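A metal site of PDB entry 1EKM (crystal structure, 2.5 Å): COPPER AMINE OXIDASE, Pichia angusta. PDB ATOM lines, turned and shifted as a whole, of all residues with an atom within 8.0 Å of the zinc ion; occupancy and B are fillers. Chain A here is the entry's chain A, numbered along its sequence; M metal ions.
Leu 409 touches the zinc ion (CD2 to ZN, 3.8 Å).
The nearest printed residue that does not touch the zinc ion is Leu 413 (4.6 Å).
The zinc ion is bound by a ring nitrogen (ND1) of His 608, at 1.9 Å.
NE2 of His 440 is bound to the zinc ion, at 2.0 Å.
The zinc ion is bound by OH of Tyr 389, 2.0 Å away.
The zinc ion is bound by NE2 of His 442, at 2.1 Å.
The zinc ion has four donor atoms within binding distance.
OD2 of Asp 614 is in hydrogen-bond range of NE2 of His 608 (3.3 Å).
The backbone carbonyl oxygen (O) of His 438 lies within hydrogen-bond range of a ring nitrogen (ND1) of His 440 (2.8 Å).
The backbone NH of His 442 is in hydrogen-bond range of the backbone carbonyl oxygen of Ile 606, 2.8 Å away.
A ring nitrogen (ND1) of His 442 is in hydrogen-bond range of the side-chain hydroxyl (OH) of Tyr 391.
The backbone carbonyl oxygen (O) of Leu 409 lies within hydrogen-bond range of the backbone NH (N) of Glu 621 (2.8 Å).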
ATOM      1  N   VAL A 287       5.173  12.732   9.513  1.00  0.00           N
ATOM      2  CA  VAL A 287       4.385  13.667   8.699  1.00  0.00           C
ATOM      3  C   VAL A 287       5.215  14.945   8.531  1.00  0.00           C
ATOM      4  O   VAL A 287       5.006  15.953   9.225  1.00  0.00           O
ATOM      5  CB  VAL A 287       3.029  13.955   9.390  1.00  0.00           C
ATOM      6  CG1 VAL A 287       2.224  14.964   8.599  1.00  0.00           C
ATOM      7  CG2 VAL A 287       2.254  12.673   9.536  1.00  0.00           C
ATOM      8  N   TYR A 289       6.440  18.381   7.161  1.00  0.00           N
ATOM      9  CA  TYR A 289       5.880  19.530   6.473  1.00  0.00           C
ATOM     10  C   TYR A 289       6.950  20.157   5.562  1.00  0.00           C
ATOM     11  O   TYR A 289       8.159  20.078   5.827  1.00  0.00           O
ATOM     12  CB  TYR A 289       5.304  20.526   7.493  1.00  0.00           C
ATOM     13  CG  TYR A 289       3.923  20.115   7.966  1.00  0.00           C
ATOM     14  CD1 TYR A 289       3.758  19.064   8.867  1.00  0.00           C
ATOM     15  CD2 TYR A 289       2.777  20.693   7.428  1.00  0.00           C
ATOM     16  CE1 TYR A 289       2.489  18.588   9.206  1.00  0.00           C
ATOM     17  CE2 TYR A 289       1.504  20.239   7.763  1.00  0.00           C
ATOM     18  CZ  TYR A 289       1.371  19.180   8.650  1.00  0.00           C
ATOM     19  OH  TYR A 289       0.123  18.659   8.920  1.00  0.00           O
ATOM     20  N   ASN A 388      -4.793  17.533  15.833  1.00  0.00           N
ATOM     21  CA  ASN A 388      -5.653  17.965  14.721  1.00  0.00           C
ATOM     22  C   ASN A 388      -6.159  16.862  13.796  1.00  0.00           C
ATOM     23  O   ASN A 388      -7.299  16.916  13.340  1.00  0.00           O
ATOM     24  CB  ASN A 388      -4.919  19.008  13.873  1.00  0.00           C
ATOM     25  CG  ASN A 388      -3.558  18.513  13.403  1.00  0.00           C
ATOM     26  OD1 ASN A 388      -2.636  18.397  14.199  1.00  0.00           O
ATOM     27  ND2 ASN A 388      -3.436  18.222  12.108  1.00  0.00           N
ATOM     28  N   TYR A 389      -5.325  15.853  13.515  1.00  0.00           N
ATOM     29  CA  TYR A 389      -5.698  14.771  12.587  1.00  0.00           C
ATOM     30  C   TYR A 389      -6.293  13.496  13.207  1.00  0.00           C
ATOM     31  O   TYR A 389      -6.067  13.206  14.382  1.00  0.00           O
ATOM     32  CB  TYR A 389      -4.472  14.341  11.802  1.00  0.00           C
ATOM     33  CG  TYR A 389      -4.187  15.116  10.545  1.00  0.00           C
ATOM     34  CD1 TYR A 389      -5.166  15.274   9.575  1.00  0.00           C
ATOM     35  CD2 TYR A 389      -2.922  15.664  10.313  1.00  0.00           C
ATOM     36  CE1 TYR A 389      -4.899  15.956   8.387  1.00  0.00           C
ATOM     37  CE2 TYR A 389      -2.641  16.344   9.127  1.00  0.00           C
ATOM     38  CZ  TYR A 389      -3.640  16.478   8.170  1.00  0.00           C
ATOM     39  OH  TYR A 389      -3.376  17.131   6.977  1.00  0.00           O
ATOM     40  N   TYR A 391      -6.593   9.321  12.307  1.00  0.00           N
ATOM     41  CA  TYR A 391      -6.163   8.269  11.410  1.00  0.00           C
ATOM     42  C   TYR A 391      -7.056   7.042  11.640  1.00  0.00           C
ATOM     43  O   TYR A 391      -7.150   6.546  12.765  1.00  0.00           O
ATOM     44  CB  TYR A 391      -4.680   7.892  11.639  1.00  0.00           C
ATOM     45  CG  TYR A 391      -3.700   8.986  11.245  1.00  0.00           C
ATOM     46  CD1 TYR A 391      -3.470  10.075  12.086  1.00  0.00           C
ATOM     47  CD2 TYR A 391      -3.018   8.933  10.022  1.00  0.00           C
ATOM     48  CE1 TYR A 391      -2.585  11.096  11.723  1.00  0.00           C
ATOM     49  CE2 TYR A 391      -2.138   9.944   9.639  1.00  0.00           C
ATOM     50  CZ  TYR A 391      -1.927  11.025  10.500  1.00  0.00           C
ATOM     51  OH  TYR A 391      -1.079  12.045  10.141  1.00  0.00           O
ATOM     52  N   LEU A 409      -7.611   8.953   6.070  1.00  0.00           N
ATOM     53  CA  LEU A 409      -7.125  10.119   6.802  1.00  0.00           C
ATOM     54  C   LEU A 409      -8.234  11.128   6.851  1.00  0.00           C
ATOM     55  O   LEU A 409      -8.843  11.444   5.836  1.00  0.00           O
ATOM     56  CB  LEU A 409      -5.901  10.739   6.103  1.00  0.00           C
ATOM     57  CG  LEU A 409      -5.435  12.081   6.711  1.00  0.00           C
ATOM     58  CD1 LEU A 409      -4.813  11.846   8.095  1.00  0.00           C
ATOM     59  CD2 LEU A 409      -4.428  12.775   5.796  1.00  0.00           C
ATOM     60  N   THR A 410      -8.516  11.631   8.055  1.00  0.00           N
ATOM     61  CA  THR A 410      -9.552  12.628   8.212  1.00  0.00           C
ATOM     62  C   THR A 410      -9.135  13.550   9.337  1.00  0.00           C
ATOM     63  O   THR A 410      -7.971  13.547   9.734  1.00  0.00           O
ATOM     64  CB  THR A 410     -10.956  11.998   8.470  1.00  0.00           C
ATOM     65  OG1 THR A 410     -11.935  13.035   8.503  1.00  0.00           O
ATOM     66  CG2 THR A 410     -10.979  11.240   9.776  1.00  0.00           C
ATOM     67  N   ILE A 412      -8.553  17.397  10.942  1.00  0.00           N
ATOM     68  CA  ILE A 412      -8.313  18.761  10.536  1.00  0.00           C
ATOM     69  C   ILE A 412      -6.883  19.074  10.123  1.00  0.00           C
ATOM     70  O   ILE A 412      -5.929  18.633  10.765  1.00  0.00           O
ATOM     71  CB  ILE A 412      -8.725  19.687  11.711  1.00  0.00           C
ATOM     72  CG1 ILE A 412     -10.178  19.389  12.065  1.00  0.00           C
ATOM     73  CG2 ILE A 412      -8.528  21.141  11.361  1.00  0.00           C
ATOM     74  CD1 ILE A 412     -10.694  20.154  13.227  1.00  0.00           C
ATOM     75  N   LEU A 413      -6.734  19.846   9.041  1.00  0.00           N
ATOM     76  CA  LEU A 413      -5.435  20.249   8.535  1.00  0.00           C
ATOM     77  C   LEU A 413      -4.644  21.056   9.558  1.00  0.00           C
ATOM     78  O   LEU A 413      -5.220  21.838  10.323  1.00  0.00           O
ATOM     79  CB  LEU A 413      -5.586  21.154   7.324  1.00  0.00           C
ATOM     80  CG  LEU A 413      -6.147  20.641   6.006  1.00  0.00           C
ATOM     81  CD1 LEU A 413      -6.540  21.818   5.143  1.00  0.00           C
ATOM     82  CD2 LEU A 413      -5.112  19.766   5.326  1.00  0.00           C
ATOM     83  N   ASN A 414      -3.328  20.870   9.574  1.00  0.00           N
ATOM     84  CA  ASN A 414      -2.520  21.705  10.450  1.00  0.00           C
ATOM     85  C   ASN A 414      -2.499  23.062   9.740  1.00  0.00           C
ATOM     86  O   ASN A 414      -2.346  23.130   8.518  1.00  0.00           O
ATOM     87  CB  ASN A 414      -1.088  21.197  10.553  1.00  0.00           C
ATOM     88  CG  ASN A 414      -0.127  22.297  10.952  1.00  0.00           C
ATOM     89  OD1 ASN A 414       0.542  22.875  10.099  1.00  0.00           O
ATOM     90  ND2 ASN A 414      -0.070  22.615  12.239  1.00  0.00           N
ATOM     91  N   HIS A 438       0.115  24.280   5.206  1.00  0.00           N
ATOM     92  CA  HIS A 438       1.405  23.881   4.642  1.00  0.00           C
ATOM     93  C   HIS A 438       1.444  22.516   3.956  1.00  0.00           C
ATOM     94  O   HIS A 438       0.785  21.560   4.393  1.00  0.00           O
ATOM     95  CB  HIS A 438       2.461  23.902   5.742  1.00  0.00           C
ATOM     96  CG  HIS A 438       2.854  25.275   6.176  1.00  0.00           C
ATOM     97  ND1 HIS A 438       3.406  25.534   7.412  1.00  0.00           N
ATOM     98  CD2 HIS A 438       2.799  26.467   5.531  1.00  0.00           C
ATOM     99  CE1 HIS A 438       3.674  26.826   7.502  1.00  0.00           C
ATOM    100  NE2 HIS A 438       3.321  27.417   6.387  1.00  0.00           N
ATOM    101  N   ASN A 439       2.236  22.415   2.885  1.00  0.00           N
ATOM    102  CA  ASN A 439       2.378  21.147   2.183  1.00  0.00           C
ATOM    103  C   ASN A 439       3.019  20.172   3.168  1.00  0.00           C
ATOM    104  O   ASN A 439       3.704  20.588   4.113  1.00  0.00           O
ATOM    105  CB  ASN A 439       3.286  21.291   0.965  1.00  0.00           C
ATOM    106  CG  ASN A 439       2.733  22.265  -0.067  1.00  0.00           C
ATOM    107  OD1 ASN A 439       1.521  22.497  -0.097  1.00  0.00           O
ATOM    108  ND2 ASN A 439       3.609  22.835  -0.905  1.00  0.00           N
ATOM    109  N   HIS A 440       2.797  18.888   2.960  1.00  0.00           N
ATOM    110  CA  HIS A 440       3.405  17.907   3.848  1.00  0.00           C
ATOM    111  C   HIS A 440       3.085  16.521   3.324  1.00  0.00           C
ATOM    112  O   HIS A 440       2.201  16.352   2.481  1.00  0.00           O
ATOM    113  CB  HIS A 440       2.824  18.059   5.253  1.00  0.00           C
ATOM    114  CG  HIS A 440       1.335  17.876   5.298  1.00  0.00           C
ATOM    115  ND1 HIS A 440       0.431  18.865   4.982  1.00  0.00           N
ATOM    116  CD2 HIS A 440       0.606  16.765   5.508  1.00  0.00           C
ATOM    117  CE1 HIS A 440      -0.800  18.323   5.000  1.00  0.00           C
ATOM    118  NE2 HIS A 440      -0.753  17.042   5.321  1.00  0.00           N
ATOM    119  N   GLN A 441       3.812  15.534   3.850  1.00  0.00           N
ATOM    120  CA  GLN A 441       3.607  14.143   3.480  1.00  0.00           C
ATOM    121  C   GLN A 441       3.139  13.379   4.716  1.00  0.00           C
ATOM    122  O   GLN A 441       3.355  13.819   5.858  1.00  0.00           O
ATOM    123  CB  GLN A 441       4.899  13.508   2.977  1.00  0.00           C
ATOM    124  CG  GLN A 441       5.637  14.260   1.871  1.00  0.00           C
ATOM    125  CD  GLN A 441       6.746  13.420   1.247  1.00  0.00           C
ATOM    126  OE1 GLN A 441       6.519  12.710   0.253  1.00  0.00           O
ATOM    127  NE2 GLN A 441       7.941  13.475   1.824  1.00  0.00           N
ATOM    128  N   HIS A 442       2.478  12.261   4.484  1.00  0.00           N
ATOM    129  CA  HIS A 442       2.034  11.383   5.561  1.00  0.00           C
ATOM    130  C   HIS A 442       2.739  10.079   5.187  1.00  0.00           C
ATOM    131  O   HIS A 442       2.367   9.430   4.199  1.00  0.00           O
ATOM    132  CB  HIS A 442       0.516  11.173   5.514  1.00  0.00           C
ATOM    133  CG  HIS A 442      -0.283  12.352   5.992  1.00  0.00           C
ATOM    134  ND1 HIS A 442      -0.623  12.565   7.310  1.00  0.00           N
ATOM    135  CD2 HIS A 442      -0.837  13.375   5.301  1.00  0.00           C
ATOM    136  CE1 HIS A 442      -1.363  13.684   7.365  1.00  0.00           C
ATOM    137  NE2 HIS A 442      -1.534  14.216   6.168  1.00  0.00           N
ATOM    138  N   ILE A 606       1.173   9.232   1.530  1.00  0.00           N
ATOM    139  CA  ILE A 606       0.754  10.194   0.512  1.00  0.00           C
ATOM    140  C   ILE A 606       1.480  11.541   0.665  1.00  0.00           C
ATOM    141  O   ILE A 606       2.082  11.835   1.704  1.00  0.00           O
ATOM    142  CB  ILE A 606      -0.754  10.487   0.628  1.00  0.00           C
ATOM    143  CG1 ILE A 606      -1.032  11.168   1.970  1.00  0.00           C
ATOM    144  CG2 ILE A 606      -1.554   9.204   0.522  1.00  0.00           C
ATOM    145  CD1 ILE A 606      -2.456  11.614   2.161  1.00  0.00           C
ATOM    146  N   THR A 607       1.419  12.343  -0.396  1.00  0.00           N
ATOM    147  CA  THR A 607       2.002  13.682  -0.369  1.00  0.00           C
ATOM    148  C   THR A 607       0.755  14.559  -0.406  1.00  0.00           C
ATOM    149  O   THR A 607       0.030  14.613  -1.405  1.00  0.00           O
ATOM    150  CB  THR A 607       2.861  13.959  -1.582  1.00  0.00           C
ATOM    151  OG1 THR A 607       4.000  13.108  -1.536  1.00  0.00           O
ATOM    152  CG2 THR A 607       3.341  15.400  -1.561  1.00  0.00           C
ATOM    153  N   HIS A 608       0.514  15.242   0.703  1.00  0.00           N
ATOM    154  CA  HIS A 608      -0.677  16.062   0.873  1.00  0.00           C
ATOM    155  C   HIS A 608      -0.529  17.530   0.481  1.00  0.00           C
ATOM    156  O   HIS A 608       0.180  18.283   1.141  1.00  0.00           O
ATOM    157  CB  HIS A 608      -1.122  15.931   2.330  1.00  0.00           C
ATOM    158  CG  HIS A 608      -2.527  16.353   2.601  1.00  0.00           C
ATOM    159  ND1 HIS A 608      -3.091  16.232   3.850  1.00  0.00           N
ATOM    160  CD2 HIS A 608      -3.454  16.874   1.749  1.00  0.00           C
ATOM    161  CE1 HIS A 608      -4.320  16.687   3.749  1.00  0.00           C
ATOM    162  NE2 HIS A 608      -4.591  17.086   2.492  1.00  0.00           N
ATOM    163  N   PHE A 609      -1.180  17.919  -0.608  1.00  0.00           N
ATOM    164  CA  PHE A 609      -1.191  19.318  -1.042  1.00  0.00           C
ATOM    165  C   PHE A 609      -2.594  19.819  -0.694  1.00  0.00           C
ATOM    166  O   PHE A 609      -3.544  19.605  -1.445  1.00  0.00           O
ATOM    167  CB  PHE A 609      -0.943  19.427  -2.547  1.00  0.00           C
ATOM    168  CG  PHE A 609       0.479  19.150  -2.929  1.00  0.00           C
ATOM    169  CD1 PHE A 609       1.491  20.033  -2.559  1.00  0.00           C
ATOM    170  CD2 PHE A 609       0.808  17.983  -3.632  1.00  0.00           C
ATOM    171  CE1 PHE A 609       2.834  19.745  -2.869  1.00  0.00           C
ATOM    172  CE2 PHE A 609       2.150  17.695  -3.942  1.00  0.00           C
ATOM    173  CZ  PHE A 609       3.160  18.580  -3.562  1.00  0.00           C
ATOM    174  N   PRO A 610      -2.730  20.512   0.441  1.00  0.00           N
ATOM    175  CA  PRO A 610      -4.031  21.027   0.875  1.00  0.00           C
ATOM    176  C   PRO A 610      -4.802  21.791  -0.179  1.00  0.00           C
ATOM    177  O   PRO A 610      -4.222  22.438  -1.051  1.00  0.00           O
ATOM    178  CB  PRO A 610      -3.678  21.900   2.072  1.00  0.00           C
ATOM    179  CG  PRO A 610      -2.380  21.335   2.580  1.00  0.00           C
ATOM    180  CD  PRO A 610      -1.645  21.029   1.294  1.00  0.00           C
ATOM    181  N   ASP A 614     -10.505  20.301   1.807  1.00  0.00           N
ATOM    182  CA  ASP A 614     -10.053  19.660   3.052  1.00  0.00           C
ATOM    183  C   ASP A 614     -10.408  20.427   4.322  1.00  0.00           C
ATOM    184  O   ASP A 614     -10.257  19.906   5.441  1.00  0.00           O
ATOM    185  CB  ASP A 614      -8.533  19.451   3.044  1.00  0.00           C
ATOM    186  CG  ASP A 614      -8.040  18.734   1.807  1.00  0.00           C
ATOM    187  OD1 ASP A 614      -8.732  17.809   1.332  1.00  0.00           O
ATOM    188  OD2 ASP A 614      -6.948  19.080   1.321  1.00  0.00           O
ATOM    189  N   MET A 618     -11.698  17.771   7.048  1.00  0.00           N
ATOM    190  CA  MET A 618     -11.386  17.061   5.811  1.00  0.00           C
ATOM    191  C   MET A 618     -12.104  15.753   5.485  1.00  0.00           C
ATOM    192  O   MET A 618     -12.249  14.894   6.338  1.00  0.00           O
ATOM    193  CB  MET A 618      -9.872  16.828   5.744  1.00  0.00           C
ATOM    194  CG  MET A 618      -9.439  15.788   4.722  1.00  0.00           C
ATOM    195  SD  MET A 618      -7.625  15.638   4.656  1.00  0.00           S
ATOM    196  CE  MET A 618      -7.318  14.940   6.210  1.00  0.00           C
ATOM    197  N   GLU A 621      -9.465  10.701   3.232  1.00  0.00           N
ATOM    198  CA  GLU A 621      -8.631  10.411   2.084  1.00  0.00           C
ATOM    199  C   GLU A 621      -8.106   8.979   2.236  1.00  0.00           C
ATOM    200  O   GLU A 621      -7.548   8.631   3.270  1.00  0.00           O
ATOM    201  CB  GLU A 621      -7.446  11.381   1.977  1.00  0.00           C
ATOM    202  CG  GLU A 621      -6.817  11.315   0.603  1.00  0.00           C
ATOM    203  CD  GLU A 621      -5.755  12.350   0.390  1.00  0.00           C
ATOM    204  OE1 GLU A 621      -6.016  13.529   0.708  1.00  0.00           O
ATOM    205  OE2 GLU A 621      -4.670  11.990  -0.102  1.00  0.00           O
HETATM  206 ZN    ZN M   1      -2.406  16.013   5.602  1.00  0.00          ZN
